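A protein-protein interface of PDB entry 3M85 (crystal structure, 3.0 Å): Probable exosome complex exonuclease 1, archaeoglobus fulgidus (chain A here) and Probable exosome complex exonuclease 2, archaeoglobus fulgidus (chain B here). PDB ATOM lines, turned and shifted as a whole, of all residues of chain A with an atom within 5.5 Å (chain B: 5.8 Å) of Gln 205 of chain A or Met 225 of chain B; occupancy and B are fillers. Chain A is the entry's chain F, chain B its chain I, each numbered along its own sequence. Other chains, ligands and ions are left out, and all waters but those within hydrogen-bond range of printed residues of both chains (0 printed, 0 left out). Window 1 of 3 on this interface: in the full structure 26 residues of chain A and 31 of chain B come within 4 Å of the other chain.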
ATOM      1  N   GLU A 100     -18.847  17.939   7.354  1.00  0.00           N
ATOM      2  CA  GLU A 100     -18.864  16.499   7.105  1.00  0.00           C
ATOM      3  C   GLU A 100     -20.234  15.832   7.285  1.00  0.00           C
ATOM      4  O   GLU A 100     -20.739  15.174   6.366  1.00  0.00           O
ATOM      5  CB  GLU A 100     -17.791  15.824   7.977  1.00  0.00           C
ATOM      6  CG  GLU A 100     -18.145  14.443   8.517  1.00  0.00           C
ATOM      7  CD  GLU A 100     -17.603  13.298   7.671  1.00  0.00           C
ATOM      8  OE1 GLU A 100     -17.619  13.411   6.420  1.00  0.00           O
ATOM      9  OE2 GLU A 100     -17.177  12.283   8.276  1.00  0.00           O
ATOM     10  N   VAL A 104     -22.482  13.850   4.421  1.00  0.00           N
ATOM     11  CA  VAL A 104     -22.921  12.460   4.384  1.00  0.00           C
ATOM     12  C   VAL A 104     -24.428  12.370   4.514  1.00  0.00           C
ATOM     13  O   VAL A 104     -25.050  11.534   3.862  1.00  0.00           O
ATOM     14  CB  VAL A 104     -22.267  11.582   5.474  1.00  0.00           C
ATOM     15  CG1 VAL A 104     -20.742  11.683   5.414  1.00  0.00           C
ATOM     16  CG2 VAL A 104     -22.807  11.947   6.869  1.00  0.00           C
ATOM     17  N   ARG A 137     -26.705  12.846  15.147  1.00  0.00           N
ATOM     18  CA  ARG A 137     -26.708  12.729  13.689  1.00  0.00           C
ATOM     19  C   ARG A 137     -27.875  11.824  13.367  1.00  0.00           C
ATOM     20  O   ARG A 137     -28.655  12.066  12.443  1.00  0.00           O
ATOM     21  CB  ARG A 137     -25.426  12.076  13.160  1.00  0.00           C
ATOM     22  CG  ARG A 137     -24.158  12.859  13.381  1.00  0.00           C
ATOM     23  CD  ARG A 137     -23.682  12.784  14.842  1.00  0.00           C
ATOM     24  NE  ARG A 137     -23.567  11.408  15.325  1.00  0.00           N
ATOM     25  CZ  ARG A 137     -22.896  10.433  14.698  1.00  0.00           C
ATOM     26  NH1 ARG A 137     -22.259  10.660  13.540  1.00  0.00           N
ATOM     27  NH2 ARG A 137     -22.865   9.214  15.235  1.00  0.00           N
ATOM     28  N   ASP A 186     -18.494   3.188  17.792  1.00  0.00           N
ATOM     29  CA  ASP A 186     -19.596   4.091  17.533  1.00  0.00           C
ATOM     30  C   ASP A 186     -19.856   3.956  16.060  1.00  0.00           C
ATOM     31  O   ASP A 186     -18.985   4.261  15.255  1.00  0.00           O
ATOM     32  CB  ASP A 186     -19.183   5.527  17.838  1.00  0.00           C
ATOM     33  CG  ASP A 186     -20.331   6.532  17.672  1.00  0.00           C
ATOM     34  OD1 ASP A 186     -20.033   7.756  17.704  1.00  0.00           O
ATOM     35  OD2 ASP A 186     -21.515   6.120  17.525  1.00  0.00           O
ATOM     36  N   MET A 187     -21.056   3.508  15.707  1.00  0.00           N
ATOM     37  CA  MET A 187     -21.374   3.154  14.336  1.00  0.00           C
ATOM     38  C   MET A 187     -22.788   3.571  13.938  1.00  0.00           C
ATOM     39  O   MET A 187     -23.748   2.842  14.184  1.00  0.00           O
ATOM     40  CB  MET A 187     -21.220   1.650  14.173  1.00  0.00           C
ATOM     41  CG  MET A 187     -21.352   1.171  12.755  1.00  0.00           C
ATOM     42  SD  MET A 187     -21.146  -0.620  12.628  1.00  0.00           S
ATOM     43  CE  MET A 187     -20.833  -0.746  10.874  1.00  0.00           C
ATOM     44  N   PRO A 188     -22.930   4.756  13.333  1.00  0.00           N
ATOM     45  CA  PRO A 188     -24.245   5.197  12.883  1.00  0.00           C
ATOM     46  C   PRO A 188     -24.695   4.592  11.537  1.00  0.00           C
ATOM     47  O   PRO A 188     -24.014   4.711  10.516  1.00  0.00           O
ATOM     48  CB  PRO A 188     -24.062   6.700  12.756  1.00  0.00           C
ATOM     49  CG  PRO A 188     -22.675   6.848  12.447  1.00  0.00           C
ATOM     50  CD  PRO A 188     -21.974   5.862  13.305  1.00  0.00           C
ATOM     51  N   PHE A 189     -25.859   3.945  11.549  1.00  0.00           N
ATOM     52  CA  PHE A 189     -26.500   3.489  10.325  1.00  0.00           C
ATOM     53  C   PHE A 189     -27.694   4.347   9.933  1.00  0.00           C
ATOM     54  O   PHE A 189     -28.280   5.065  10.749  1.00  0.00           O
ATOM     55  CB  PHE A 189     -27.015   2.065  10.491  1.00  0.00           C
ATOM     56  CG  PHE A 189     -25.946   1.050  10.710  1.00  0.00           C
ATOM     57  CD1 PHE A 189     -25.479   0.787  11.983  1.00  0.00           C
ATOM     58  CD2 PHE A 189     -25.422   0.342   9.643  1.00  0.00           C
ATOM     59  CE1 PHE A 189     -24.522  -0.153  12.187  1.00  0.00           C
ATOM     60  CE2 PHE A 189     -24.451  -0.608   9.844  1.00  0.00           C
ATOM     61  CZ  PHE A 189     -24.000  -0.854  11.111  1.00  0.00           C
ATOM     62  N   LEU A 203     -26.776   5.042   5.050  1.00  0.00           N
ATOM     63  CA  LEU A 203     -25.701   5.753   5.705  1.00  0.00           C
ATOM     64  C   LEU A 203     -24.938   4.766   6.542  1.00  0.00           C
ATOM     65  O   LEU A 203     -25.540   3.872   7.129  1.00  0.00           O
ATOM     66  CB  LEU A 203     -26.237   6.896   6.543  1.00  0.00           C
ATOM     67  CG  LEU A 203     -25.134   7.760   7.132  1.00  0.00           C
ATOM     68  CD1 LEU A 203     -25.498   9.221   6.981  1.00  0.00           C
ATOM     69  CD2 LEU A 203     -24.869   7.430   8.581  1.00  0.00           C
ATOM     70  N   LEU A 204     -23.615   4.915   6.592  1.00  0.00           N
ATOM     71  CA  LEU A 204     -22.778   3.937   7.270  1.00  0.00           C
ATOM     72  C   LEU A 204     -21.449   4.541   7.645  1.00  0.00           C
ATOM     73  O   LEU A 204     -20.600   4.708   6.788  1.00  0.00           O
ATOM     74  CB  LEU A 204     -22.557   2.717   6.351  1.00  0.00           C
ATOM     75  CG  LEU A 204     -21.923   1.390   6.820  1.00  0.00           C
ATOM     76  CD1 LEU A 204     -20.479   1.308   6.451  1.00  0.00           C
ATOM     77  CD2 LEU A 204     -22.057   1.173   8.304  1.00  0.00           C
ATOM     78  N   GLN A 205     -21.263   4.864   8.919  1.00  0.00           N
ATOM     79  CA  GLN A 205     -19.952   5.270   9.424  1.00  0.00           C
ATOM     80  C   GLN A 205     -19.568   4.439  10.632  1.00  0.00           C
ATOM     81  O   GLN A 205     -20.430   4.013  11.395  1.00  0.00           O
ATOM     82  CB  GLN A 205     -19.979   6.724   9.837  1.00  0.00           C
ATOM     83  CG  GLN A 205     -20.240   7.701   8.705  1.00  0.00           C
ATOM     84  CD  GLN A 205     -20.114   9.152   9.156  1.00  0.00           C
ATOM     85  OE1 GLN A 205     -19.002   9.667   9.352  1.00  0.00           O
ATOM     86  NE2 GLN A 205     -21.257   9.815   9.335  1.00  0.00           N
ATOM     87  N   MET A 206     -18.285   4.183  10.813  1.00  0.00           N
ATOM     88  CA  MET A 206     -17.857   3.650  12.098  1.00  0.00           C
ATOM     89  C   MET A 206     -16.493   4.179  12.549  1.00  0.00           C
ATOM     90  O   MET A 206     -15.620   4.488  11.733  1.00  0.00           O
ATOM     91  CB  MET A 206     -17.984   2.102  12.198  1.00  0.00           C
ATOM     92  CG  MET A 206     -16.741   1.264  11.894  1.00  0.00           C
ATOM     93  SD  MET A 206     -15.441   1.164  13.167  1.00  0.00           S
ATOM     94  CE  MET A 206     -16.270   0.226  14.430  1.00  0.00           C
ATOM     95  N   ASP A 207     -16.357   4.321  13.864  1.00  0.00           N
ATOM     96  CA  ASP A 207     -15.115   4.710  14.518  1.00  0.00           C
ATOM     97  C   ASP A 207     -15.033   3.735  15.653  1.00  0.00           C
ATOM     98  O   ASP A 207     -16.056   3.422  16.254  1.00  0.00           O
ATOM     99  CB  ASP A 207     -15.213   6.121  15.092  1.00  0.00           C
ATOM    100  CG  ASP A 207     -14.537   7.166  14.212  1.00  0.00           C
ATOM    101  OD1 ASP A 207     -13.375   7.517  14.520  1.00  0.00           O
ATOM    102  OD2 ASP A 207     -15.157   7.650  13.229  1.00  0.00           O
ATOM    103  N   VAL A 215     -18.899  -6.324  13.316  1.00  0.00           N
ATOM    104  CA  VAL A 215     -19.517  -5.483  12.276  1.00  0.00           C
ATOM    105  C   VAL A 215     -20.819  -6.135  11.814  1.00  0.00           C
ATOM    106  O   VAL A 215     -21.903  -5.537  11.910  1.00  0.00           O
ATOM    107  CB  VAL A 215     -18.594  -5.223  11.030  1.00  0.00           C
ATOM    108  CG1 VAL A 215     -19.402  -4.696   9.853  1.00  0.00           C
ATOM    109  CG2 VAL A 215     -17.470  -4.257  11.364  1.00  0.00           C
ATOM    110  N   ARG B 111      -8.919   9.351  11.521  1.00  0.00           N
ATOM    111  CA  ARG B 111      -9.765   8.376  12.192  1.00  0.00           C
ATOM    112  C   ARG B 111      -9.069   7.038  12.364  1.00  0.00           C
ATOM    113  O   ARG B 111      -8.977   6.518  13.480  1.00  0.00           O
ATOM    114  CB  ARG B 111     -11.056   8.188  11.411  1.00  0.00           C
ATOM    115  CG  ARG B 111     -12.263   8.657  12.154  1.00  0.00           C
ATOM    116  CD  ARG B 111     -13.283   9.258  11.245  1.00  0.00           C
ATOM    117  NE  ARG B 111     -14.237   8.255  10.844  1.00  0.00           N
ATOM    118  CZ  ARG B 111     -15.040   8.381   9.799  1.00  0.00           C
ATOM    119  NH1 ARG B 111     -15.882   7.412   9.509  1.00  0.00           N
ATOM    120  NH2 ARG B 111     -14.997   9.473   9.045  1.00  0.00           N
ATOM    121  N   LEU B 212     -16.924   3.185  -0.814  1.00  0.00           N
ATOM    122  CA  LEU B 212     -16.949   2.611   0.528  1.00  0.00           C
ATOM    123  C   LEU B 212     -15.508   2.508   0.953  1.00  0.00           C
ATOM    124  O   LEU B 212     -14.659   2.086   0.182  1.00  0.00           O
ATOM    125  CB  LEU B 212     -17.523   1.207   0.528  1.00  0.00           C
ATOM    126  CG  LEU B 212     -18.225   0.728   1.808  1.00  0.00           C
ATOM    127  CD1 LEU B 212     -17.874  -0.718   2.145  1.00  0.00           C
ATOM    128  CD2 LEU B 212     -17.903   1.612   2.957  1.00  0.00           C
ATOM    129  N   THR B 213     -15.222   2.904   2.182  1.00  0.00           N
ATOM    130  CA  THR B 213     -13.871   2.840   2.699  1.00  0.00           C
ATOM    131  C   THR B 213     -13.912   2.067   3.998  1.00  0.00           C
ATOM    132  O   THR B 213     -14.713   2.381   4.872  1.00  0.00           O
ATOM    133  CB  THR B 213     -13.344   4.230   2.996  1.00  0.00           C
ATOM    134  OG1 THR B 213     -13.278   4.986   1.778  1.00  0.00           O
ATOM    135  CG2 THR B 213     -11.965   4.154   3.645  1.00  0.00           C
ATOM    136  N   ILE B 214     -13.061   1.053   4.114  1.00  0.00           N
ATOM    137  CA  ILE B 214     -12.909   0.292   5.336  1.00  0.00           C
ATOM    138  C   ILE B 214     -11.431   0.331   5.770  1.00  0.00           C
ATOM    139  O   ILE B 214     -10.530   0.080   4.960  1.00  0.00           O
ATOM    140  CB  ILE B 214     -13.351  -1.129   5.098  1.00  0.00           C
ATOM    141  CG1 ILE B 214     -14.808  -1.144   4.669  1.00  0.00           C
ATOM    142  CG2 ILE B 214     -13.116  -1.987   6.317  1.00  0.00           C
ATOM    143  CD1 ILE B 214     -15.351  -2.523   4.549  1.00  0.00           C
ATOM    144  N   THR B 215     -11.186   0.670   7.035  1.00  0.00           N
ATOM    145  CA  THR B 215      -9.834   0.780   7.583  1.00  0.00           C
ATOM    146  C   THR B 215      -9.635  -0.280   8.663  1.00  0.00           C
ATOM    147  O   THR B 215     -10.509  -0.471   9.508  1.00  0.00           O
ATOM    148  CB  THR B 215      -9.616   2.165   8.253  1.00  0.00           C
ATOM    149  OG1 THR B 215      -9.696   3.214   7.281  1.00  0.00           O
ATOM    150  CG2 THR B 215      -8.266   2.234   8.948  1.00  0.00           C
ATOM    151  N   VAL B 222     -11.696  -4.198  12.340  1.00  0.00           N
ATOM    152  CA  VAL B 222     -12.192  -3.033  11.627  1.00  0.00           C
ATOM    153  C   VAL B 222     -12.162  -1.843  12.584  1.00  0.00           C
ATOM    154  O   VAL B 222     -12.608  -1.932  13.731  1.00  0.00           O
ATOM    155  CB  VAL B 222     -13.604  -3.241  11.133  1.00  0.00           C
ATOM    156  CG1 VAL B 222     -14.162  -1.936  10.598  1.00  0.00           C
ATOM    157  CG2 VAL B 222     -13.630  -4.308  10.059  1.00  0.00           C
ATOM    158  N   VAL B 223     -11.649  -0.718  12.113  1.00  0.00           N
ATOM    159  CA  VAL B 223     -11.289   0.366  13.014  1.00  0.00           C
ATOM    160  C   VAL B 223     -11.944   1.705  12.587  1.00  0.00           C
ATOM    161  O   VAL B 223     -12.115   2.627  13.396  1.00  0.00           O
ATOM    162  CB  VAL B 223      -9.726   0.426  13.123  1.00  0.00           C
ATOM    163  CG1 VAL B 223      -9.162   1.685  12.508  1.00  0.00           C
ATOM    164  CG2 VAL B 223      -9.275   0.221  14.560  1.00  0.00           C
ATOM    165  N   ALA B 224     -12.335   1.771  11.311  1.00  0.00           N
ATOM    166  CA  ALA B 224     -12.969   2.940  10.706  1.00  0.00           C
ATOM    167  C   ALA B 224     -13.623   2.526   9.406  1.00  0.00           C
ATOM    168  O   ALA B 224     -13.007   1.865   8.594  1.00  0.00           O
ATOM    169  CB  ALA B 224     -11.947   3.996  10.411  1.00  0.00           C
ATOM    170  N   MET B 225     -14.866   2.921   9.190  1.00  0.00           N
ATOM    171  CA  MET B 225     -15.468   2.708   7.892  1.00  0.00           C
ATOM    172  C   MET B 225     -16.185   3.966   7.449  1.00  0.00           C
ATOM    173  O   MET B 225     -16.544   4.798   8.253  1.00  0.00           O
ATOM    174  CB  MET B 225     -16.436   1.543   7.938  1.00  0.00           C
ATOM    175  CG  MET B 225     -15.898   0.285   8.600  1.00  0.00           C
ATOM    176  SD  MET B 225     -17.247  -0.915   8.634  1.00  0.00           S
ATOM    177  CE  MET B 225     -17.576  -0.832   6.899  1.00  0.00           C
ATOM    178  N   GLN B 226     -16.410   4.102   6.158  1.00  0.00           N
ATOM    179  CA  GLN B 226     -17.052   5.300   5.659  1.00  0.00           C
ATOM    180  C   GLN B 226     -17.669   5.065   4.282  1.00  0.00           C
ATOM    181  O   GLN B 226     -16.960   4.915   3.287  1.00  0.00           O
ATOM    182  CB  GLN B 226     -16.016   6.416   5.598  1.00  0.00           C
ATOM    183  CG  GLN B 226     -16.490   7.652   4.895  1.00  0.00           C
ATOM    184  CD  GLN B 226     -17.152   8.640   5.818  1.00  0.00           C
ATOM    185  OE1 GLN B 226     -16.885   8.661   7.019  1.00  0.00           O
ATOM    186  NE2 GLN B 226     -18.000   9.489   5.258  1.00  0.00           N
ATOM    187  N   LYS B 227     -18.997   4.998   4.235  1.00  0.00           N
ATOM    188  CA  LYS B 227     -19.716   5.028   2.962  1.00  0.00           C
ATOM    189  C   LYS B 227     -19.863   6.476   2.544  1.00  0.00           C
ATOM    190  O   LYS B 227     -20.062   7.351   3.388  1.00  0.00           O
ATOM    191  CB  LYS B 227     -21.098   4.401   3.079  1.00  0.00           C
ATOM    192  CG  LYS B 227     -21.965   4.562   1.828  1.00  0.00           C
ATOM    193  CD  LYS B 227     -23.388   4.096   2.112  1.00  0.00           C
ATOM    194  CE  LYS B 227     -24.315   4.316   0.931  1.00  0.00           C
ATOM    195  NZ  LYS B 227     -24.570   5.756   0.634  1.00  0.00           N
ATOM    196  N   PHE B 238     -22.339  -5.183   0.959  1.00  0.00           N
ATOM    197  CA  PHE B 238     -21.469  -4.675   1.989  1.00  0.00           C
ATOM    198  C   PHE B 238     -20.749  -5.819   2.696  1.00  0.00           C
ATOM    199  O   PHE B 238     -19.541  -5.743   2.974  1.00  0.00           O
ATOM    200  CB  PHE B 238     -22.189  -3.807   3.015  1.00  0.00           C
ATOM    201  CG  PHE B 238     -21.343  -3.530   4.215  1.00  0.00           C
ATOM    202  CD1 PHE B 238     -20.292  -2.633   4.136  1.00  0.00           C
ATOM    203  CD2 PHE B 238     -21.536  -4.236   5.397  1.00  0.00           C
ATOM    204  CE1 PHE B 238     -19.483  -2.416   5.220  1.00  0.00           C
ATOM    205  CE2 PHE B 238     -20.718  -4.017   6.495  1.00  0.00           C
ATOM    206  CZ  PHE B 238     -19.692  -3.109   6.405  1.00  0.00           C
ATOM    207  N   LEU B 242     -16.663  -6.418   2.866  1.00  0.00           N
ATOM    208  CA  LEU B 242     -16.064  -6.306   4.184  1.00  0.00           C
ATOM    209  C   LEU B 242     -14.834  -7.172   4.212  1.00  0.00           C
ATOM    210  O   LEU B 242     -13.758  -6.752   4.640  1.00  0.00           O
ATOM    211  CB  LEU B 242     -17.033  -6.840   5.244  1.00  0.00           C
ATOM    212  CG  LEU B 242     -17.013  -6.358   6.716  1.00  0.00           C
ATOM    213  CD1 LEU B 242     -17.443  -7.467   7.679  1.00  0.00           C
ATOM    214  CD2 LEU B 242     -15.680  -5.761   7.154  1.00  0.00           C
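The side-chain amide oxygen of Gln 205 of chain A sits close to the side-chain carboxylate of Glu 100 of chain A (3.4 Å).
The guanidinium group (NH1) of Arg 111 of chain B is in hydrogen-bond range of the backbone carbonyl oxygen (O) of Met 225 of chain B, at 3.0 Å.
O of Thr 213 of chain B sits at hydrogen-bond distance from N of Gln 226 of chain B (2.7 Å).
The backbone NH (N) of Val 223 of chain B lies within hydrogen-bond range of the backbone carbonyl oxygen (O) of Thr 215 of chain B, 2.9 Å away.
The backbone NH (N) of Gln 205 of chain A lies within hydrogen-bond range of the backbone carbonyl oxygen (O) of Pro 188 of chain A.
The guanidinium group of Arg 111 of chain B is in hydrogen-bond range of the side-chain amide oxygen of Gln 226 of chain B, at 2.9 Å.
Glu 100 of chain A touches Gln 226 of chain B.
CG1 of Val 104 of chain A touches NE2 of Gln 226 of chain B (3.5 Å).
CD1 of Leu 204 of chain A touches CE of Met 225 of chain B, 3.6 Å away.
Leu 204 of chain A touches Gln 226 of chain B (O to CA, 3.8 Å).
OE1 of Gln 205 of chain A touches NH1 of Arg 111 of chain B (3.9 Å).
Gln 205 of chain A touches Met 225 of chain B (CA to O, 3.6 Å).
Met 206 of chain A touches Arg 111 of chain B (O to NH1, 3.7 Å).
CA of Asp 207 of chain A touches O of Val 223 of chain B (3.8 Å).
Val 215 of chain A touches Phe 238 of chain B (CG1 to CE2, 3.7 Å).
OE1 of Gln 205 of chain A lies close to OE1 of Gln 226 of chain B, at 3.3 Å.
O of Met 206 of chain A is in hydrogen-bond range of N of Met 225 of chain B (3.1 Å).
NE of Arg 111 of chain B lies within salt-bridge range of OD2 of Asp 207 of chain A, at 2.6 Å.
The backbone carbonyl oxygen (O) of Val 223 of chain B sits close to the side-chain sulfur (SD) of Met 206 of chain A, at 3.6 Å.
NH2 of Arg 111 of chain B is in salt-bridge range of OE2 of Glu 100 of chain A (3.6 Å).
N of Ala 224 of chain B is in hydrogen-bond range of SD of Met 206 of chain A (3.7 Å).
The backbone carbonyl oxygen (O) of Leu 204 of chain A lies within hydrogen-bond range of the backbone NH (N) of Lys 227 of chain B (3.0 Å).
Hydrophobic or aromatic side chains of chain A within 4 Å of the printed part of chain B: Val 104, Leu 204, Met 206 and Val 215.
Hydrophobic or aromatic side chains of chain B that line the printed part of chain A: Ala 224, Met 225 and Phe 238.
Along chain B the printed residues that touch a printed residue of chain A span positions 111 to 238.
Among the printed residues, 16 pairs touch across the chains.
Gln 205 of chain A touches three residues of chain B.
Of the printed residues of chain A, Ala 224 of chain B touches Met 206.
Of the printed residues of chain A, Val 223 of chain B touches Met 206 and Asp 207.
Of the printed residues of chain A, Lys 227 of chain B touches Leu 204 (3.0 Å).
Phe 189 of chain A touches none of the printed residues of chain B.
The nearest printed residue of chain B that does not touch Val 215 of chain A is Val 222 of chain B (4.004 Å).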
